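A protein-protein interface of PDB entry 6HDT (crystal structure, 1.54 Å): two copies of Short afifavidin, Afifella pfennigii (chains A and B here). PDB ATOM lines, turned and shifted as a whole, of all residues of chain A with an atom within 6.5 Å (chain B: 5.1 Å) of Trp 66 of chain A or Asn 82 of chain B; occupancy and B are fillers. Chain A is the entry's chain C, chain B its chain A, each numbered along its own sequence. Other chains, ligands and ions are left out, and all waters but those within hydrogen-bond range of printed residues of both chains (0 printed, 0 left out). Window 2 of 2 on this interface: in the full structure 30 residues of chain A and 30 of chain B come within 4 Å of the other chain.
Printed residues of chain B that touch a printed residue of chain A: Ala 75, Asp 77, Asn 82, Asn 84 and Val 86.
Hydrophobic or aromatic side chains of chain B that line the printed part of chain A: Ala 75 and Val 86.
Among the printed residues, 8 pairs touch across the chains.
Among the printed residues, no Asp or Glu carboxylate lies within 4 Å of a Lys or Arg side-chain nitrogen of the other chain.
Among the printed residues, pairs that only touch across the chains: Phe 69 of chain A with Asn 84 of chain B (3.2 Å), Trp 66 of chain A with Asn 82 of chain B (3.3 Å), Trp 66 of chain A with Asp 77 of chain B (3.5 Å), Phe 69 of chain A with Val 86 of chain B (3.7 Å), Leu 64 of chain A with Ala 75 of chain B (3.8 Å), Trp 66 of chain A with Val 86 of chain B (3.9 Å) and Ile 70 of chain A with Val 86 of chain B (3.95 Å).
Of chain B, only Asp 77 (3.5 Å), Asn 82 (3.3 Å), Asn 84 (3.1 Å) and Val 86 (3.9 Å) come within 4 Å of Trp 66 of chain A.
Asn 82 of chain B touches one residue of chain A.
Of the printed residues of chain A, Val 86 of chain B touches Trp 66, Phe 69 and Ile 70.
Printed residues of chain A within 4 Å of Asn 84 of chain B: Trp 66 and Phe 69.
Of the printed residues of chain B, Ile 70 of chain A touches Val 86.
Of the printed residues of chain A, Ala 75 of chain B touches Leu 64.
Printed residues of chain B within 4 Å of Leu 64 of chain A: Ala 75.
Trp 76 of chain B touches none of the printed residues of chain A.
The nearest printed residue of chain A that does not touch Asn 82 of chain B is Asn 39 of chain A (7.3 Å).
No position is printed for both chains.
Of the 8 pairs that touch across the chains among the printed residues, none has its exchanged pair printed and touching as well.
NE1 of Trp 66 of chain A sits close to OD1 of Asn 84 of chain B (3.4 Å).
The side-chain sulfur of Cys 54 of chain B forms a disulfide with the side-chain sulfur of Cys 83 of chain B (2.1 Å).
The side-chain amide nitrogen of Asn 82 of chain B lies close to the backbone NH of Asn 84 of chain B, 2.8 Å away.
OD1 of Asn 82 of chain B lies close to OD1 of Asp 77 of chain B (2.8 Å).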
ATOM      1  N   SER A  10     -14.658   5.866 -28.249  1.00  0.00           N
ATOM      2  CA  SER A  10     -13.463   6.188 -27.477  1.00  0.00           C
ATOM      3  C   SER A  10     -12.758   7.443 -28.029  1.00  0.00           C
ATOM      4  O   SER A  10     -12.404   8.346 -27.263  1.00  0.00           O
ATOM      5  CB  SER A  10     -12.508   5.008 -27.476  1.00  0.00           C
ATOM      6  OG  SER A  10     -11.464   5.259 -26.567  1.00  0.00           O
ATOM      7  N   ALA A  13     -14.893  10.538 -27.331  1.00  0.00           N
ATOM      8  CA  ALA A  13     -14.846  10.905 -25.918  1.00  0.00           C
ATOM      9  C   ALA A  13     -13.547  11.584 -25.570  1.00  0.00           C
ATOM     10  O   ALA A  13     -13.462  12.317 -24.597  1.00  0.00           O
ATOM     11  CB  ALA A  13     -15.053   9.687 -25.029  1.00  0.00           C
ATOM     12  N   PHE A  14     -12.531  11.314 -26.366  1.00  0.00           N
ATOM     13  CA  PHE A  14     -11.265  11.974 -26.197  1.00  0.00           C
ATOM     14  C   PHE A  14     -11.329  13.388 -26.743  1.00  0.00           C
ATOM     15  O   PHE A  14     -10.677  14.268 -26.229  1.00  0.00           O
ATOM     16  CB  PHE A  14     -10.158  11.164 -26.875  1.00  0.00           C
ATOM     17  CG  PHE A  14      -8.796  11.679 -26.588  1.00  0.00           C
ATOM     18  CD1 PHE A  14      -8.266  11.575 -25.309  1.00  0.00           C
ATOM     19  CD2 PHE A  14      -8.057  12.287 -27.582  1.00  0.00           C
ATOM     20  CE1 PHE A  14      -7.018  12.068 -25.036  1.00  0.00           C
ATOM     21  CE2 PHE A  14      -6.794  12.778 -27.314  1.00  0.00           C
ATOM     22  CZ  PHE A  14      -6.277  12.676 -26.039  1.00  0.00           C
ATOM     23  N   ASN A  39     -10.482   1.067 -24.753  1.00  0.00           N
ATOM     24  CA  ASN A  39      -9.600   2.167 -24.316  1.00  0.00           C
ATOM     25  C   ASN A  39      -8.207   2.184 -24.953  1.00  0.00           C
ATOM     26  O   ASN A  39      -7.391   3.060 -24.625  1.00  0.00           O
ATOM     27  CB  ASN A  39      -9.372   2.140 -22.791  1.00  0.00           C
ATOM     28  CG  ASN A  39     -10.648   2.137 -21.984  1.00  0.00           C
ATOM     29  OD1 ASN A  39     -10.651   1.644 -20.854  1.00  0.00           O
ATOM     30  ND2 ASN A  39     -11.727   2.691 -22.531  1.00  0.00           N
ATOM     31  N   LEU A  64      -3.311   3.836 -23.245  1.00  0.00           N
ATOM     32  CA  LEU A  64      -4.749   3.724 -22.917  1.00  0.00           C
ATOM     33  C   LEU A  64      -5.364   5.070 -22.699  1.00  0.00           C
ATOM     34  O   LEU A  64      -4.695   6.015 -22.363  1.00  0.00           O
ATOM     35  CB  LEU A  64      -4.962   2.899 -21.648  1.00  0.00           C
ATOM     36  CG  LEU A  64      -4.435   1.457 -21.654  1.00  0.00           C
ATOM     37  CD1 LEU A  64      -4.408   0.870 -20.252  1.00  0.00           C
ATOM     38  CD2 LEU A  64      -5.252   0.555 -22.561  1.00  0.00           C
ATOM     39  N   THR A  65      -6.699   5.141 -22.867  1.00  0.00           N
ATOM     40  CA  THR A  65      -7.432   6.357 -22.587  1.00  0.00           C
ATOM     41  C   THR A  65      -8.657   6.079 -21.746  1.00  0.00           C
ATOM     42  O   THR A  65      -9.158   4.965 -21.696  1.00  0.00           O
ATOM     43  CB  THR A  65      -7.939   7.066 -23.872  1.00  0.00           C
ATOM     44  OG1 THR A  65      -8.826   6.204 -24.584  1.00  0.00           O
ATOM     45  CG2 THR A  65      -6.790   7.420 -24.763  1.00  0.00           C
ATOM     46  N   TRP A  66      -9.102   7.123 -21.055  1.00  0.00           N
ATOM     47  CA  TRP A  66     -10.363   7.119 -20.421  1.00  0.00           C
ATOM     48  C   TRP A  66     -10.919   8.517 -20.582  1.00  0.00           C
ATOM     49  O   TRP A  66     -10.338   9.479 -20.113  1.00  0.00           O
ATOM     50  CB  TRP A  66     -10.318   6.748 -18.927  1.00  0.00           C
ATOM     51  CG  TRP A  66     -11.716   6.771 -18.457  1.00  0.00           C
ATOM     52  CD1 TRP A  66     -12.362   7.795 -17.799  1.00  0.00           C
ATOM     53  CD2 TRP A  66     -12.710   5.805 -18.767  1.00  0.00           C
ATOM     54  NE1 TRP A  66     -13.690   7.483 -17.628  1.00  0.00           N
ATOM     55  CE2 TRP A  66     -13.934   6.270 -18.222  1.00  0.00           C
ATOM     56  CE3 TRP A  66     -12.688   4.578 -19.442  1.00  0.00           C
ATOM     57  CZ2 TRP A  66     -15.127   5.535 -18.318  1.00  0.00           C
ATOM     58  CZ3 TRP A  66     -13.880   3.843 -19.537  1.00  0.00           C
ATOM     59  CH2 TRP A  66     -15.077   4.330 -18.977  1.00  0.00           C
ATOM     60  N   GLY A  67     -12.075   8.630 -21.211  1.00  0.00           N
ATOM     61  CA  GLY A  67     -12.629   9.961 -21.437  1.00  0.00           C
ATOM     62  C   GLY A  67     -11.630  10.830 -22.193  1.00  0.00           C
ATOM     63  O   GLY A  67     -11.156  10.444 -23.261  1.00  0.00           O
ATOM     64  N   ASN A  68     -11.296  12.001 -21.652  1.00  0.00           N
ATOM     65  CA  ASN A  68     -10.346  12.883 -22.333  1.00  0.00           C
ATOM     66  C   ASN A  68      -8.941  12.741 -21.786  1.00  0.00           C
ATOM     67  O   ASN A  68      -8.112  13.577 -22.071  1.00  0.00           O
ATOM     68  CB  ASN A  68     -10.787  14.350 -22.289  1.00  0.00           C
ATOM     69  CG  ASN A  68     -10.716  14.959 -20.891  1.00  0.00           C
ATOM     70  OD1 ASN A  68     -11.183  14.363 -19.917  1.00  0.00           O
ATOM     71  ND2 ASN A  68     -10.113  16.151 -20.782  1.00  0.00           N
ATOM     72  N   PHE A  69      -8.699  11.700 -20.995  1.00  0.00           N
ATOM     73  CA  PHE A  69      -7.363  11.435 -20.430  1.00  0.00           C
ATOM     74  C   PHE A  69      -6.653  10.356 -21.207  1.00  0.00           C
ATOM     75  O   PHE A  69      -7.282   9.413 -21.721  1.00  0.00           O
ATOM     76  CB  PHE A  69      -7.520  11.030 -18.967  1.00  0.00           C
ATOM     77  CG  PHE A  69      -8.292  12.032 -18.161  1.00  0.00           C
ATOM     78  CD1 PHE A  69      -7.897  13.363 -18.180  1.00  0.00           C
ATOM     79  CD2 PHE A  69      -9.375  11.674 -17.378  1.00  0.00           C
ATOM     80  CE1 PHE A  69      -8.571  14.325 -17.454  1.00  0.00           C
ATOM     81  CE2 PHE A  69     -10.069  12.634 -16.654  1.00  0.00           C
ATOM     82  CZ  PHE A  69      -9.648  13.956 -16.672  1.00  0.00           C
ATOM     83  N   ILE A  70      -5.320  10.454 -21.270  1.00  0.00           N
ATOM     84  CA  ILE A  70      -4.564   9.537 -22.075  1.00  0.00           C
ATOM     85  C   ILE A  70      -3.202   9.332 -21.434  1.00  0.00           C
ATOM     86  O   ILE A  70      -2.670  10.220 -20.819  1.00  0.00           O
ATOM     87  CB  ILE A  70      -4.377  10.065 -23.511  1.00  0.00           C
ATOM     88  CG1 ILE A  70      -3.682   9.041 -24.419  1.00  0.00           C
ATOM     89  CG2 ILE A  70      -3.592  11.375 -23.522  1.00  0.00           C
ATOM     90  CD1 ILE A  70      -3.944   9.322 -25.889  1.00  0.00           C
ATOM     91  N   CYS B  54     -10.082   3.574  -6.376  1.00  0.00           N
ATOM     92  CA  CYS B  54      -9.826   2.352  -7.198  1.00  0.00           C
ATOM     93  C   CYS B  54      -8.802   1.420  -6.555  1.00  0.00           C
ATOM     94  O   CYS B  54      -7.848   0.945  -7.190  1.00  0.00           O
ATOM     95  CB  CYS B  54      -9.416   2.745  -8.623  1.00  0.00           C
ATOM     96  SG  CYS B  54     -10.796   3.526  -9.484  1.00  0.00           S
ATOM     97  N   TYR B  59      -6.401  -3.618 -12.428  1.00  0.00           N
ATOM     98  CA  TYR B  59      -6.622  -2.793 -13.617  1.00  0.00           C
ATOM     99  C   TYR B  59      -5.641  -3.180 -14.719  1.00  0.00           C
ATOM    100  O   TYR B  59      -4.463  -3.513 -14.454  1.00  0.00           O
ATOM    101  CB  TYR B  59      -6.512  -1.316 -13.268  1.00  0.00           C
ATOM    102  CG  TYR B  59      -7.663  -0.862 -12.419  1.00  0.00           C
ATOM    103  CD1 TYR B  59      -7.672  -1.053 -11.043  1.00  0.00           C
ATOM    104  CD2 TYR B  59      -8.781  -0.272 -13.007  1.00  0.00           C
ATOM    105  CE1 TYR B  59      -8.772  -0.668 -10.260  1.00  0.00           C
ATOM    106  CE2 TYR B  59      -9.856   0.131 -12.229  1.00  0.00           C
ATOM    107  CZ  TYR B  59      -9.854  -0.080 -10.865  1.00  0.00           C
ATOM    108  OH  TYR B  59     -10.936   0.331 -10.109  1.00  0.00           O
ATOM    109  N   ALA B  75      -5.355   2.804 -17.133  1.00  0.00           N
ATOM    110  CA  ALA B  75      -6.581   3.594 -17.126  1.00  0.00           C
ATOM    111  C   ALA B  75      -7.495   3.080 -15.993  1.00  0.00           C
ATOM    112  O   ALA B  75      -7.788   1.873 -15.934  1.00  0.00           O
ATOM    113  CB  ALA B  75      -7.255   3.442 -18.466  1.00  0.00           C
ATOM    114  N   TRP B  76      -7.944   3.967 -15.097  1.00  0.00           N
ATOM    115  CA  TRP B  76      -8.612   3.518 -13.868  1.00  0.00           C
ATOM    116  C   TRP B  76     -10.100   3.256 -14.097  1.00  0.00           C
ATOM    117  O   TRP B  76     -10.948   3.940 -13.540  1.00  0.00           O
ATOM    118  CB  TRP B  76      -8.334   4.490 -12.716  1.00  0.00           C
ATOM    119  CG  TRP B  76      -6.856   4.549 -12.434  1.00  0.00           C
ATOM    120  CD1 TRP B  76      -5.993   5.517 -12.803  1.00  0.00           C
ATOM    121  CD2 TRP B  76      -6.079   3.542 -11.771  1.00  0.00           C
ATOM    122  NE1 TRP B  76      -4.672   5.178 -12.412  1.00  0.00           N
ATOM    123  CE2 TRP B  76      -4.728   3.987 -11.750  1.00  0.00           C
ATOM    124  CE3 TRP B  76      -6.404   2.341 -11.126  1.00  0.00           C
ATOM    125  CZ2 TRP B  76      -3.714   3.239 -11.168  1.00  0.00           C
ATOM    126  CZ3 TRP B  76      -5.380   1.598 -10.568  1.00  0.00           C
ATOM    127  CH2 TRP B  76      -4.070   2.071 -10.566  1.00  0.00           C
ATOM    128  N   ASP B  77     -10.388   2.239 -14.918  1.00  0.00           N
ATOM    129  CA  ASP B  77     -11.723   1.710 -15.077  1.00  0.00           C
ATOM    130  C   ASP B  77     -11.650   0.188 -15.211  1.00  0.00           C
ATOM    131  O   ASP B  77     -10.792  -0.352 -15.906  1.00  0.00           O
ATOM    132  CB  ASP B  77     -12.403   2.323 -16.287  1.00  0.00           C
ATOM    133  CG  ASP B  77     -13.812   1.800 -16.476  1.00  0.00           C
ATOM    134  OD1 ASP B  77     -14.697   2.138 -15.645  1.00  0.00           O
ATOM    135  OD2 ASP B  77     -14.031   1.037 -17.443  1.00  0.00           O
ATOM    136  N   THR B  80     -15.461  -3.138 -11.479  1.00  0.00           N
ATOM    137  CA  THR B  80     -15.683  -2.864 -10.070  1.00  0.00           C
ATOM    138  C   THR B  80     -15.808  -1.365  -9.777  1.00  0.00           C
ATOM    139  O   THR B  80     -16.761  -0.940  -9.117  1.00  0.00           O
ATOM    140  CB  THR B  80     -14.510  -3.455  -9.250  1.00  0.00           C
ATOM    141  OG1 THR B  80     -14.561  -4.878  -9.376  1.00  0.00           O
ATOM    142  CG2 THR B  80     -14.614  -3.097  -7.797  1.00  0.00           C
ATOM    143  N   ALA B  81     -14.853  -0.583 -10.266  1.00  0.00           N
ATOM    144  CA  ALA B  81     -14.791   0.855  -9.992  1.00  0.00           C
ATOM    145  C   ALA B  81     -14.071   1.671 -11.052  1.00  0.00           C
ATOM    146  O   ALA B  81     -13.148   1.220 -11.710  1.00  0.00           O
ATOM    147  CB  ALA B  81     -14.139   1.111  -8.643  1.00  0.00           C
ATOM    148  N   ASN B  82     -14.470   2.926 -11.106  1.00  0.00           N
ATOM    149  CA  ASN B  82     -13.941   3.902 -12.030  1.00  0.00           C
ATOM    150  C   ASN B  82     -13.521   5.123 -11.236  1.00  0.00           C
ATOM    151  O   ASN B  82     -14.270   5.629 -10.372  1.00  0.00           O
ATOM    152  CB  ASN B  82     -15.008   4.290 -13.055  1.00  0.00           C
ATOM    153  CG  ASN B  82     -14.485   5.239 -14.138  1.00  0.00           C
ATOM    154  OD1 ASN B  82     -14.188   4.833 -15.256  1.00  0.00           O
ATOM    155  ND2 ASN B  82     -14.410   6.507 -13.814  1.00  0.00           N
ATOM    156  N   CYS B  83     -12.334   5.618 -11.556  1.00  0.00           N
ATOM    157  CA  CYS B  83     -11.821   6.849 -10.957  1.00  0.00           C
ATOM    158  C   CYS B  83     -11.612   8.009 -11.966  1.00  0.00           C
ATOM    159  O   CYS B  83     -11.116   9.071 -11.592  1.00  0.00           O
ATOM    160  CB  CYS B  83     -10.537   6.521 -10.185  1.00  0.00           C
ATOM    161  SG  CYS B  83     -10.895   5.509  -8.741  1.00  0.00           S
ATOM    162  N   ASN B  84     -11.951   7.793 -13.240  1.00  0.00           N
ATOM    163  CA  ASN B  84     -11.906   8.848 -14.267  1.00  0.00           C
ATOM    164  C   ASN B  84     -10.530   9.504 -14.355  1.00  0.00           C
ATOM    165  O   ASN B  84     -10.356  10.704 -14.179  1.00  0.00           O
ATOM    166  CB  ASN B  84     -13.002   9.882 -14.009  1.00  0.00           C
ATOM    167  CG  ASN B  84     -13.170  10.831 -15.164  1.00  0.00           C
ATOM    168  OD1 ASN B  84     -12.908  10.474 -16.301  1.00  0.00           O
ATOM    169  ND2 ASN B  84     -13.621  12.054 -14.876  1.00  0.00           N
ATOM    170  N   SER B  85      -9.532   8.666 -14.590  1.00  0.00           N
ATOM    171  CA  SER B  85      -8.147   9.071 -14.486  1.00  0.00           C
ATOM    172  C   SER B  85      -7.296   8.031 -15.181  1.00  0.00           C
ATOM    173  O   SER B  85      -7.735   6.901 -15.388  1.00  0.00           O
ATOM    174  CB  SER B  85      -7.731   9.133 -13.016  1.00  0.00           C
ATOM    175  OG  SER B  85      -7.990   7.889 -12.384  1.00  0.00           O
ATOM    176  N   VAL B  86      -6.074   8.434 -15.507  1.00  0.00           N
ATOM    177  CA  VAL B  86      -5.092   7.571 -16.144  1.00  0.00           C
ATOM    178  C   VAL B  86      -3.729   7.887 -15.550  1.00  0.00           C
ATOM    179  O   VAL B  86      -3.376   9.045 -15.455  1.00  0.00           O
ATOM    180  CB  VAL B  86      -5.012   7.835 -17.664  1.00  0.00           C
ATOM    181  CG1 VAL B  86      -3.896   7.025 -18.303  1.00  0.00           C
ATOM    182  CG2 VAL B  86      -6.341   7.573 -18.331  1.00  0.00           C
